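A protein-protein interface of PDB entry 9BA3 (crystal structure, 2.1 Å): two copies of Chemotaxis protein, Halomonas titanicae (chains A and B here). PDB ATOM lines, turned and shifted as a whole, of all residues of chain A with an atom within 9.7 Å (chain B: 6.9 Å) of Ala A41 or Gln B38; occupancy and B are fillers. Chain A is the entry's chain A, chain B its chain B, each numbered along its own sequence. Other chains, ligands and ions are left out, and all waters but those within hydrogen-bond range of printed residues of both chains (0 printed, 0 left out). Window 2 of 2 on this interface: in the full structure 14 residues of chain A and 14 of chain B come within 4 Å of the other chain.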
ATOM      1  N   ASN A  33      37.592  16.427   1.287  1.00  0.00           N
ATOM      2  CA  ASN A  33      36.182  16.488   1.674  1.00  0.00           C
ATOM      3  C   ASN A  33      35.670  15.131   2.139  1.00  0.00           C
ATOM      4  O   ASN A  33      34.920  15.047   3.118  1.00  0.00           O
ATOM      5  CB  ASN A  33      35.335  17.046   0.541  1.00  0.00           C
ATOM      6  CG  ASN A  33      35.013  18.511   0.744  1.00  0.00           C
ATOM      7  OD1 ASN A  33      35.536  19.155   1.657  1.00  0.00           O
ATOM      8  ND2 ASN A  33      34.151  19.048  -0.108  1.00  0.00           N
ATOM      9  N   SER A  35      37.302  13.219   3.671  1.00  0.00           N
ATOM     10  CA  SER A  35      37.937  13.043   4.970  1.00  0.00           C
ATOM     11  C   SER A  35      37.065  13.585   6.100  1.00  0.00           C
ATOM     12  O   SER A  35      37.218  13.163   7.253  1.00  0.00           O
ATOM     13  CB  SER A  35      39.312  13.719   4.992  1.00  0.00           C
ATOM     14  OG  SER A  35      40.238  13.087   4.121  1.00  0.00           O
ATOM     15  N   LEU A  36      36.184  14.544   5.809  1.00  0.00           N
ATOM     16  CA  LEU A  36      35.478  15.270   6.855  1.00  0.00           C
ATOM     17  C   LEU A  36      33.993  14.969   6.963  1.00  0.00           C
ATOM     18  O   LEU A  36      33.287  15.728   7.632  1.00  0.00           O
ATOM     19  CB  LEU A  36      35.624  16.768   6.635  1.00  0.00           C
ATOM     20  CG  LEU A  36      36.883  17.506   7.088  1.00  0.00           C
ATOM     21  CD1 LEU A  36      38.146  17.072   6.349  1.00  0.00           C
ATOM     22  CD2 LEU A  36      36.588  18.964   6.881  1.00  0.00           C
ATOM     23  N   SER A  37      33.477  13.902   6.357  1.00  0.00           N
ATOM     24  CA  SER A  37      32.033  13.707   6.468  1.00  0.00           C
ATOM     25  C   SER A  37      31.642  13.414   7.916  1.00  0.00           C
ATOM     26  O   SER A  37      30.822  14.126   8.510  1.00  0.00           O
ATOM     27  CB  SER A  37      31.571  12.589   5.537  1.00  0.00           C
ATOM     28  OG  SER A  37      32.059  11.331   5.964  1.00  0.00           O
ATOM     29  N   GLN A  38      32.259  12.399   8.521  1.00  0.00           N
ATOM     30  CA  GLN A  38      31.935  12.053   9.900  1.00  0.00           C
ATOM     31  C   GLN A  38      32.692  12.923  10.899  1.00  0.00           C
ATOM     32  O   GLN A  38      32.151  13.288  11.950  1.00  0.00           O
ATOM     33  CB  GLN A  38      32.227  10.575  10.150  1.00  0.00           C
ATOM     34  CG  GLN A  38      31.555  10.032  11.390  1.00  0.00           C
ATOM     35  CD  GLN A  38      31.908   8.584  11.654  1.00  0.00           C
ATOM     36  OE1 GLN A  38      31.301   7.934  12.506  1.00  0.00           O
ATOM     37  NE2 GLN A  38      32.911   8.076  10.941  1.00  0.00           N
ATOM     38  N   ASP A  39      33.955  13.239  10.603  1.00  0.00           N
ATOM     39  CA  ASP A  39      34.764  14.020  11.532  1.00  0.00           C
ATOM     40  C   ASP A  39      34.204  15.422  11.739  1.00  0.00           C
ATOM     41  O   ASP A  39      34.352  15.992  12.824  1.00  0.00           O
ATOM     42  CB  ASP A  39      36.206  14.087  11.035  1.00  0.00           C
ATOM     43  CG  ASP A  39      36.841  12.713  10.900  1.00  0.00           C
ATOM     44  OD1 ASP A  39      37.217  12.119  11.933  1.00  0.00           O
ATOM     45  OD2 ASP A  39      36.941  12.213   9.762  1.00  0.00           O
ATOM     46  N   LEU A  40      33.571  15.996  10.712  1.00  0.00           N
ATOM     47  CA  LEU A  40      32.967  17.316  10.863  1.00  0.00           C
ATOM     48  C   LEU A  40      31.706  17.256  11.715  1.00  0.00           C
ATOM     49  O   LEU A  40      31.477  18.135  12.554  1.00  0.00           O
ATOM     50  CB  LEU A  40      32.655  17.899   9.490  1.00  0.00           C
ATOM     51  CG  LEU A  40      32.268  19.364   9.380  1.00  0.00           C
ATOM     52  CD1 LEU A  40      33.317  20.220  10.063  1.00  0.00           C
ATOM     53  CD2 LEU A  40      32.127  19.719   7.909  1.00  0.00           C
ATOM     54  N   ALA A  41      30.868  16.236  11.506  1.00  0.00           N
ATOM     55  CA  ALA A  41      29.641  16.119  12.289  1.00  0.00           C
ATOM     56  C   ALA A  41      29.944  15.923  13.769  1.00  0.00           C
ATOM     57  O   ALA A  41      29.294  16.530  14.628  1.00  0.00           O
ATOM     58  CB  ALA A  41      28.783  14.974  11.755  1.00  0.00           C
ATOM     59  N   ILE A  42      30.937  15.091  14.091  1.00  0.00           N
ATOM     60  CA  ILE A  42      31.271  14.848  15.491  1.00  0.00           C
ATOM     61  C   ILE A  42      31.979  16.055  16.091  1.00  0.00           C
ATOM     62  O   ILE A  42      31.814  16.361  17.278  1.00  0.00           O
ATOM     63  CB  ILE A  42      32.108  13.564  15.634  1.00  0.00           C
ATOM     64  CG1 ILE A  42      31.295  12.352  15.179  1.00  0.00           C
ATOM     65  CG2 ILE A  42      32.568  13.378  17.071  1.00  0.00           C
ATOM     66  CD1 ILE A  42      29.994  12.189  15.930  1.00  0.00           C
ATOM     67  N   SER A  43      32.796  16.749  15.294  1.00  0.00           N
ATOM     68  CA  SER A  43      33.450  17.953  15.797  1.00  0.00           C
ATOM     69  C   SER A  43      32.418  19.010  16.179  1.00  0.00           C
ATOM     70  O   SER A  43      32.548  19.672  17.214  1.00  0.00           O
ATOM     71  CB  SER A  43      34.423  18.496  14.748  1.00  0.00           C
ATOM     72  OG  SER A  43      35.472  17.573  14.492  1.00  0.00           O
ATOM     73  N   GLU A  44      31.366  19.156  15.369  1.00  0.00           N
ATOM     74  CA  GLU A  44      30.310  20.112  15.690  1.00  0.00           C
ATOM     75  C   GLU A  44      29.553  19.707  16.950  1.00  0.00           C
ATOM     76  O   GLU A  44      29.240  20.557  17.793  1.00  0.00           O
ATOM     77  CB  GLU A  44      29.339  20.244  14.518  1.00  0.00           C
ATOM     78  CG  GLU A  44      28.164  21.162  14.804  1.00  0.00           C
ATOM     79  CD  GLU A  44      27.216  21.280  13.627  1.00  0.00           C
ATOM     80  OE1 GLU A  44      27.524  20.722  12.552  1.00  0.00           O
ATOM     81  OE2 GLU A  44      26.169  21.940  13.777  1.00  0.00           O
ATOM     82  N   SER A  45      29.220  18.423  17.088  1.00  0.00           N
ATOM     83  CA  SER A  45      28.490  18.006  18.280  1.00  0.00           C
ATOM     84  C   SER A  45      29.358  18.108  19.528  1.00  0.00           C
ATOM     85  O   SER A  45      28.844  18.401  20.613  1.00  0.00           O
ATOM     86  CB  SER A  45      27.946  16.587  18.107  1.00  0.00           C
ATOM     87  OG  SER A  45      28.995  15.653  17.928  1.00  0.00           O
ATOM     88  N   LEU A  46      30.668  17.890  19.398  1.00  0.00           N
ATOM     89  CA  LEU A  46      31.554  18.027  20.550  1.00  0.00           C
ATOM     90  C   LEU A  46      31.673  19.484  20.981  1.00  0.00           C
ATOM     91  O   LEU A  46      31.535  19.804  22.169  1.00  0.00           O
ATOM     92  CB  LEU A  46      32.932  17.449  20.226  1.00  0.00           C
ATOM     93  CG  LEU A  46      33.974  17.574  21.336  1.00  0.00           C
ATOM     94  CD1 LEU A  46      33.450  16.902  22.593  1.00  0.00           C
ATOM     95  CD2 LEU A  46      35.319  16.972  20.910  1.00  0.00           C
ATOM     96  N   ALA A  47      31.894  20.390  20.025  1.00  0.00           N
ATOM     97  CA  ALA A  47      32.029  21.801  20.370  1.00  0.00           C
ATOM     98  C   ALA A  47      30.760  22.336  21.015  1.00  0.00           C
ATOM     99  O   ALA A  47      30.823  23.140  21.951  1.00  0.00           O
ATOM    100  CB  ALA A  47      32.381  22.617  19.129  1.00  0.00           C
ATOM    101  N   ASN A  48      29.599  21.877  20.555  1.00  0.00           N
ATOM    102  CA  ASN A  48      28.328  22.340  21.091  1.00  0.00           C
ATOM    103  C   ASN A  48      27.763  21.422  22.156  1.00  0.00           C
ATOM    104  O   ASN A  48      26.616  21.613  22.570  1.00  0.00           O
ATOM    105  CB  ASN A  48      27.304  22.503  19.969  1.00  0.00           C
ATOM    106  CG  ASN A  48      27.601  23.681  19.091  1.00  0.00           C
ATOM    107  OD1 ASN A  48      27.358  24.823  19.479  1.00  0.00           O
ATOM    108  ND2 ASN A  48      28.149  23.420  17.906  1.00  0.00           N
ATOM    109  N   SER A  49      28.554  20.473  22.645  1.00  0.00           N
ATOM    110  CA  SER A  49      28.055  19.482  23.588  1.00  0.00           C
ATOM    111  C   SER A  49      27.529  20.137  24.856  1.00  0.00           C
ATOM    112  O   SER A  49      28.217  20.949  25.480  1.00  0.00           O
ATOM    113  CB  SER A  49      29.168  18.497  23.942  1.00  0.00           C
ATOM    114  OG  SER A  49      28.776  17.692  25.037  1.00  0.00           O
ATOM    115  N   LEU A  75      34.070   8.966  21.566  1.00  0.00           N
ATOM    116  CA  LEU A  75      34.071   9.629  20.268  1.00  0.00           C
ATOM    117  C   LEU A  75      35.256   9.186  19.421  1.00  0.00           C
ATOM    118  O   LEU A  75      35.125   8.997  18.206  1.00  0.00           O
ATOM    119  CB  LEU A  75      34.098  11.146  20.445  1.00  0.00           C
ATOM    120  CG  LEU A  75      32.837  11.794  21.019  1.00  0.00           C
ATOM    121  CD1 LEU A  75      33.007  13.305  21.080  1.00  0.00           C
ATOM    122  CD2 LEU A  75      31.612  11.406  20.206  1.00  0.00           C
ATOM    123  N   GLN A  78      34.730   5.998  17.601  1.00  0.00           N
ATOM    124  CA  GLN A  78      33.846   6.102  16.446  1.00  0.00           C
ATOM    125  C   GLN A  78      34.558   6.687  15.226  1.00  0.00           C
ATOM    126  O   GLN A  78      34.350   6.215  14.103  1.00  0.00           O
ATOM    127  CB  GLN A  78      32.611   6.927  16.814  1.00  0.00           C
ATOM    128  CG  GLN A  78      31.779   7.335  15.619  1.00  0.00           C
ATOM    129  CD  GLN A  78      30.500   8.061  15.980  1.00  0.00           C
ATOM    130  OE1 GLN A  78      30.178   8.275  17.154  1.00  0.00           O
ATOM    131  NE2 GLN A  78      29.768   8.468  14.957  1.00  0.00           N
ATOM    132  N   LEU A  79      35.405   7.701  15.423  1.00  0.00           N
ATOM    133  CA  LEU A  79      35.985   8.459  14.317  1.00  0.00           C
ATOM    134  C   LEU A  79      37.281   7.903  13.742  1.00  0.00           C
ATOM    135  O   LEU A  79      37.560   8.150  12.562  1.00  0.00           O
ATOM    136  CB  LEU A  79      36.248   9.899  14.746  1.00  0.00           C
ATOM    137  CG  LEU A  79      35.037  10.789  14.994  1.00  0.00           C
ATOM    138  CD1 LEU A  79      35.517  12.153  15.443  1.00  0.00           C
ATOM    139  CD2 LEU A  79      34.210  10.882  13.723  1.00  0.00           C
ATOM    140  N   LEU A  84      41.500  14.300  19.807  1.00  0.00           N
ATOM    141  CA  LEU A  84      40.374  15.205  19.976  1.00  0.00           C
ATOM    142  C   LEU A  84      40.799  16.295  20.946  1.00  0.00           C
ATOM    143  O   LEU A  84      41.535  16.026  21.900  1.00  0.00           O
ATOM    144  CB  LEU A  84      39.141  14.466  20.515  1.00  0.00           C
ATOM    145  CG  LEU A  84      38.506  13.408  19.610  1.00  0.00           C
ATOM    146  CD1 LEU A  84      37.382  12.703  20.343  1.00  0.00           C
ATOM    147  CD2 LEU A  84      37.980  14.043  18.334  1.00  0.00           C
ATOM    148  N   TYR A 129      33.354  26.795  11.283  1.00  0.00           N
ATOM    149  CA  TYR A 129      34.522  25.960  11.490  1.00  0.00           C
ATOM    150  C   TYR A 129      35.591  26.309  10.465  1.00  0.00           C
ATOM    151  O   TYR A 129      35.360  27.064   9.519  1.00  0.00           O
ATOM    152  CB  TYR A 129      34.153  24.476  11.458  1.00  0.00           C
ATOM    153  CG  TYR A 129      34.027  23.849  10.106  1.00  0.00           C
ATOM    154  CD1 TYR A 129      32.831  23.863   9.386  1.00  0.00           C
ATOM    155  CD2 TYR A 129      35.119  23.220   9.550  1.00  0.00           C
ATOM    156  CE1 TYR A 129      32.758  23.262   8.117  1.00  0.00           C
ATOM    157  CE2 TYR A 129      35.059  22.630   8.315  1.00  0.00           C
ATOM    158  CZ  TYR A 129      33.891  22.646   7.602  1.00  0.00           C
ATOM    159  OH  TYR A 129      33.888  22.004   6.389  1.00  0.00           O
ATOM    160  N   VAL A 147      40.319  20.177  12.776  1.00  0.00           N
ATOM    161  CA  VAL A 147      38.957  20.627  12.505  1.00  0.00           C
ATOM    162  C   VAL A 147      38.558  21.519  13.678  1.00  0.00           C
ATOM    163  O   VAL A 147      38.159  21.032  14.733  1.00  0.00           O
ATOM    164  CB  VAL A 147      37.994  19.452  12.327  1.00  0.00           C
ATOM    165  CG1 VAL A 147      36.591  19.947  12.022  1.00  0.00           C
ATOM    166  CG2 VAL A 147      38.478  18.518  11.222  1.00  0.00           C
ATOM    167  N   TYR A 149      36.029  23.672  15.282  1.00  0.00           N
ATOM    168  CA  TYR A 149      34.602  23.979  15.275  1.00  0.00           C
ATOM    169  C   TYR A 149      34.232  24.753  16.537  1.00  0.00           C
ATOM    170  O   TYR A 149      34.601  24.351  17.645  1.00  0.00           O
ATOM    171  CB  TYR A 149      33.770  22.697  15.176  1.00  0.00           C
ATOM    172  CG  TYR A 149      32.504  22.871  14.370  1.00  0.00           C
ATOM    173  CD1 TYR A 149      31.474  23.682  14.827  1.00  0.00           C
ATOM    174  CD2 TYR A 149      32.346  22.237  13.143  1.00  0.00           C
ATOM    175  CE1 TYR A 149      30.318  23.854  14.088  1.00  0.00           C
ATOM    176  CE2 TYR A 149      31.192  22.408  12.392  1.00  0.00           C
ATOM    177  CZ  TYR A 149      30.181  23.217  12.872  1.00  0.00           C
ATOM    178  OH  TYR A 149      29.026  23.398  12.147  1.00  0.00           O
ATOM    179  N   ALA A 164      36.239  22.991  19.591  1.00  0.00           N
ATOM    180  CA  ALA A 164      36.555  21.575  19.725  1.00  0.00           C
ATOM    181  C   ALA A 164      36.594  20.926  18.350  1.00  0.00           C
ATOM    182  O   ALA A 164      36.108  21.483  17.362  1.00  0.00           O
ATOM    183  CB  ALA A 164      35.547  20.867  20.638  1.00  0.00           C
ATOM    184  N   GLY A 165      37.169  19.731  18.300  1.00  0.00           N
ATOM    185  CA  GLY A 165      37.241  18.997  17.051  1.00  0.00           C
ATOM    186  C   GLY A 165      38.333  17.940  17.102  1.00  0.00           C
ATOM    187  O   GLY A 165      38.814  17.573  18.172  1.00  0.00           O
ATOM    188  N   ALA A 166      38.724  17.486  15.916  1.00  0.00           N
ATOM    189  CA  ALA A 166      39.665  16.388  15.776  1.00  0.00           C
ATOM    190  C   ALA A 166      40.922  16.846  15.051  1.00  0.00           C
ATOM    191  O   ALA A 166      40.918  17.834  14.312  1.00  0.00           O
ATOM    192  CB  ALA A 166      39.037  15.215  15.016  1.00  0.00           C
ATOM    193  N   SER B  35      21.796   8.432   1.853  1.00  0.00           N
ATOM    194  CA  SER B  35      21.527   9.861   2.000  1.00  0.00           C
ATOM    195  C   SER B  35      21.801  10.399   3.403  1.00  0.00           C
ATOM    196  O   SER B  35      22.067  11.597   3.549  1.00  0.00           O
ATOM    197  CB  SER B  35      20.081  10.158   1.609  1.00  0.00           C
ATOM    198  OG  SER B  35      19.174   9.454   2.438  1.00  0.00           O
ATOM    199  N   LEU B  36      21.744   9.561   4.440  1.00  0.00           N
ATOM    200  CA  LEU B  36      21.692  10.070   5.816  1.00  0.00           C
ATOM    201  C   LEU B  36      23.051   9.941   6.506  1.00  0.00           C
ATOM    202  O   LEU B  36      23.243   9.211   7.476  1.00  0.00           O
ATOM    203  CB  LEU B  36      20.572   9.373   6.594  1.00  0.00           C
ATOM    204  CG  LEU B  36      20.324   7.857   6.570  1.00  0.00           C
ATOM    205  CD1 LEU B  36      21.224   7.047   7.507  1.00  0.00           C
ATOM    206  CD2 LEU B  36      18.855   7.583   6.882  1.00  0.00           C
ATOM    207  N   SER B  37      24.000  10.732   6.003  1.00  0.00           N
ATOM    208  CA  SER B  37      25.351  10.717   6.552  1.00  0.00           C
ATOM    209  C   SER B  37      25.386  11.262   7.977  1.00  0.00           C
ATOM    210  O   SER B  37      25.889  10.599   8.892  1.00  0.00           O
ATOM    211  CB  SER B  37      26.286  11.524   5.649  1.00  0.00           C
ATOM    212  OG  SER B  37      25.962  12.903   5.695  1.00  0.00           O
ATOM    213  N   GLN B  38      24.818  12.450   8.197  1.00  0.00           N
ATOM    214  CA  GLN B  38      24.937  13.083   9.508  1.00  0.00           C
ATOM    215  C   GLN B  38      24.023  12.447  10.546  1.00  0.00           C
ATOM    216  O   GLN B  38      24.418  12.291  11.707  1.00  0.00           O
ATOM    217  CB  GLN B  38      24.622  14.574   9.409  1.00  0.00           C
ATOM    218  CG  GLN B  38      25.078  15.363  10.621  1.00  0.00           C
ATOM    219  CD  GLN B  38      24.665  16.819  10.558  1.00  0.00           C
ATOM    220  OE1 GLN B  38      25.116  17.634  11.361  1.00  0.00           O
ATOM    221  NE2 GLN B  38      23.771  17.146   9.633  1.00  0.00           N
ATOM    222  N   ASP B  39      22.798  12.090  10.157  1.00  0.00           N
ATOM    223  CA  ASP B  39      21.872  11.497  11.114  1.00  0.00           C
ATOM    224  C   ASP B  39      22.378  10.154  11.622  1.00  0.00           C
ATOM    225  O   ASP B  39      22.120   9.785  12.774  1.00  0.00           O
ATOM    226  CB  ASP B  39      20.490  11.352  10.480  1.00  0.00           C
ATOM    227  CG  ASP B  39      19.912  12.685  10.045  1.00  0.00           C
ATOM    228  OD1 ASP B  39      19.630  13.524  10.923  1.00  0.00           O
ATOM    229  OD2 ASP B  39      19.754  12.901   8.826  1.00  0.00           O
ATOM    230  N   LEU B  40      23.099   9.414  10.778  1.00  0.00           N
ATOM    231  CA  LEU B  40      23.665   8.139  11.199  1.00  0.00           C
ATOM    232  C   LEU B  40      24.837   8.343  12.150  1.00  0.00           C
ATOM    233  O   LEU B  40      24.954   7.638  13.159  1.00  0.00           O
ATOM    234  CB  LEU B  40      24.092   7.341   9.969  1.00  0.00           C
ATOM    235  CG  LEU B  40      24.472   5.876  10.165  1.00  0.00           C
ATOM    236  CD1 LEU B  40      23.374   5.121  10.903  1.00  0.00           C
ATOM    237  CD2 LEU B  40      24.751   5.242   8.813  1.00  0.00           C
ATOM    238  N   ALA B  41      25.708   9.312  11.853  1.00  0.00           N
ATOM    239  CA  ALA B  41      26.857   9.563  12.718  1.00  0.00           C
ATOM    240  C   ALA B  41      26.419   9.995  14.111  1.00  0.00           C
ATOM    241  O   ALA B  41      26.984   9.544  15.113  1.00  0.00           O
ATOM    242  CB  ALA B  41      27.766  10.619  12.090  1.00  0.00           C
ATOM    243  N   ILE B  42      25.402  10.854  14.195  1.00  0.00           N
ATOM    244  CA  ILE B  42      24.949  11.328  15.499  1.00  0.00           C
ATOM    245  C   ILE B  42      24.195  10.227  16.239  1.00  0.00           C
ATOM    246  O   ILE B  42      24.311  10.094  17.463  1.00  0.00           O
ATOM    247  CB  ILE B  42      24.097  12.600  15.335  1.00  0.00           C
ATOM    248  CG1 ILE B  42      24.930  13.733  14.725  1.00  0.00           C
ATOM    249  CG2 ILE B  42      23.522  13.035  16.674  1.00  0.00           C
ATOM    250  CD1 ILE B  42      26.157  14.091  15.521  1.00  0.00           C
ATOM    251  N   SER B  43      23.430   9.407  15.513  1.00  0.00           N
ATOM    252  CA  SER B  43      22.730   8.297  16.155  1.00  0.00           C
ATOM    253  C   SER B  43      23.714   7.329  16.803  1.00  0.00           C
ATOM    254  O   SER B  43      23.451   6.803  17.890  1.00  0.00           O
ATOM    255  CB  SER B  43      21.847   7.563  15.144  1.00  0.00           C
ATOM    256  OG  SER B  43      20.809   8.398  14.657  1.00  0.00           O
ATOM    257  N   GLU B  44      24.853   7.077  16.147  1.00  0.00           N
ATOM    258  CA  GLU B  44      25.863   6.193  16.728  1.00  0.00           C
ATOM    259  C   GLU B  44      26.473   6.796  17.989  1.00  0.00           C
ATOM    260  O   GLU B  44      26.624   6.101  19.003  1.00  0.00           O
ATOM    261  CB  GLU B  44      26.957   5.887  15.703  1.00  0.00           C
ATOM    262  CG  GLU B  44      28.095   5.033  16.249  1.00  0.00           C
ATOM    263  CD  GLU B  44      29.152   4.730  15.207  1.00  0.00           C
ATOM    264  OE1 GLU B  44      28.951   5.094  14.029  1.00  0.00           O
ATOM    265  OE2 GLU B  44      30.183   4.122  15.564  1.00  0.00           O
ATOM    266  N   GLN B  78      21.556  20.666  15.834  1.00  0.00           N
ATOM    267  CA  GLN B  78      22.452  20.325  14.736  1.00  0.00           C
ATOM    268  C   GLN B  78      21.712  19.568  13.642  1.00  0.00           C
ATOM    269  O   GLN B  78      21.928  19.805  12.449  1.00  0.00           O
ATOM    270  CB  GLN B  78      23.628  19.502  15.262  1.00  0.00           C
ATOM    271  CG  GLN B  78      24.465  18.868  14.179  1.00  0.00           C
ATOM    272  CD  GLN B  78      25.685  18.152  14.722  1.00  0.00           C
ATOM    273  OE1 GLN B  78      25.914  18.115  15.932  1.00  0.00           O
ATOM    274  NE2 GLN B  78      26.487  17.592  13.822  1.00  0.00           N
ATOM    275  N   LEU B  79      20.850  18.643  14.031  1.00  0.00           N
ATOM    276  CA  LEU B  79      20.158  17.801  13.077  1.00  0.00           C
ATOM    277  C   LEU B  79      18.856  18.456  12.628  1.00  0.00           C
ATOM    278  O   LEU B  79      18.450  19.513  13.113  1.00  0.00           O
ATOM    279  CB  LEU B  79      19.877  16.431  13.687  1.00  0.00           C
ATOM    280  CG  LEU B  79      21.099  15.560  13.964  1.00  0.00           C
ATOM    281  CD1 LEU B  79      20.664  14.258  14.611  1.00  0.00           C
ATOM    282  CD2 LEU B  79      21.884  15.298  12.686  1.00  0.00           C
ATOM    283  N   ASP B  80      18.207  17.813  11.665  1.00  0.00           N
ATOM    284  CA  ASP B  80      16.920  18.257  11.146  1.00  0.00           C
ATOM    285  C   ASP B  80      15.955  17.076  11.209  1.00  0.00           C
ATOM    286  O   ASP B  80      15.513  16.542  10.195  1.00  0.00           O
ATOM    287  CB  ASP B  80      17.023  18.812   9.729  1.00  0.00           C
ATOM    288  CG  ASP B  80      15.689  19.353   9.218  1.00  0.00           C
ATOM    289  OD1 ASP B  80      14.729  19.459  10.015  1.00  0.00           O
ATOM    290  OD2 ASP B  80      15.598  19.663   8.010  1.00  0.00           O
ATOM    291  N   LEU B 176      17.524  15.050   2.377  1.00  0.00           N
ATOM    292  CA  LEU B 176      18.741  14.246   2.374  1.00  0.00           C
ATOM    293  C   LEU B 176      18.986  13.606   1.014  1.00  0.00           C
ATOM    294  O   LEU B 176      20.142  13.388   0.635  1.00  0.00           O
ATOM    295  CB  LEU B 176      18.667  13.167   3.458  1.00  0.00           C
ATOM    296  CG  LEU B 176      18.573  13.651   4.906  1.00  0.00           C
ATOM    297  CD1 LEU B 176      18.428  12.472   5.848  1.00  0.00           C
ATOM    298  CD2 LEU B 176      19.783  14.490   5.283  1.00  0.00           C
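The side-chain amide nitrogen of Gln A78 is in hydrogen-bond range of the backbone carbonyl oxygen of Ala B41 (3.0 Å). The backbone carbonyl oxygen (O) of Ala A41 sits at hydrogen-bond distance from the side-chain amide nitrogen (NE2) of Gln B78.
O of Glu A44 is in hydrogen-bond range of ND2 of Asn A48, at 3.1 Å. The backbone carbonyl oxygen (O) of Ile A42 is in hydrogen-bond range of the side-chain hydroxyl (OG) of Ser A45, at 3.0 Å. OE1 of Glu A44 is in hydrogen-bond range of OH of Tyr A149, at 3.1 Å. The side-chain amide oxygen (OE1) of Gln B38 lies within hydrogen-bond range of the side-chain amide nitrogen (NE2) of Gln B78, 2.8 Å away. The side-chain amide nitrogen of Gln A78 lies within hydrogen-bond range of the side-chain amide oxygen of Gln A38, 2.9 Å away. The backbone carbonyl oxygen (O) of Ala A41 lies within hydrogen-bond range of the side-chain hydroxyl (OG) of Ser A45 (3.4 Å).
Ala B41 touches Gln A38 (CB to CG, 3.9 Å). Gln A38 touches Glu B44. Gln B38 touches Ala A41 (CG to CB, 3.9 Å). Glu A44 touches Gln B78. Gln B78 touches Ser A45. Glu B44 touches Gln A78.
Of chain B, only Gln B38 and Gln B78 come within 4 Å of Ala A41. Of chain A, only Ala A41 (3.9 Å) comes within 4 Å of Gln B38. No residue of chain A comes within 4 Å of Asp B39. Ala B41 touches just these residues of chain A: Gln A38 and Gln A78. Printed residues of chain B within 4 Å of Gln A78: Ala B41 and Glu B44. Of the printed residues of chain A, Gln B78 touches Ala A41 (3.1 Å), Glu A44 (3.5 Å) and Ser A45 (3.3 Å). Printed residues of chain B within 4 Å of Gln A38: Ala B41 and Glu B44. Of the printed residues of chain A, Glu B44 touches Gln A38 and Gln A78. Ala A166 touches none of the printed residues of chain B. Asn A33 touches none of the printed residues of chain B. The nearest residue of chain B that does not touch Ala A41 is Ile B42 (4.1 Å). The nearest residue of chain A that does not touch Gln B38 is Glu A44 (4.1 Å).
Of the 14 printed residues of chain B, 4 touch a printed residue of chain A. Printed residues of chain B that touch a printed residue of chain A: Gln B38, Ala B41, Glu B44 and Gln B78. Among the printed residues, no Asp or Glu carboxylate lies within 4 Å of a Lys or Arg side-chain nitrogen of the other chain.
Gln A38 touches Ala B41, and with the chains exchanged Ala A41 touches Gln B38. Gln A38 touches Glu B44, but with the chains exchanged Glu A44 does not touch Gln B38 (4.1 Å). Ala A41 touches Gln B78, and with the chains exchanged Gln A78 touches Ala B41. Glu A44 touches Gln B78, and with the chains exchanged Gln A78 touches Glu B44.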
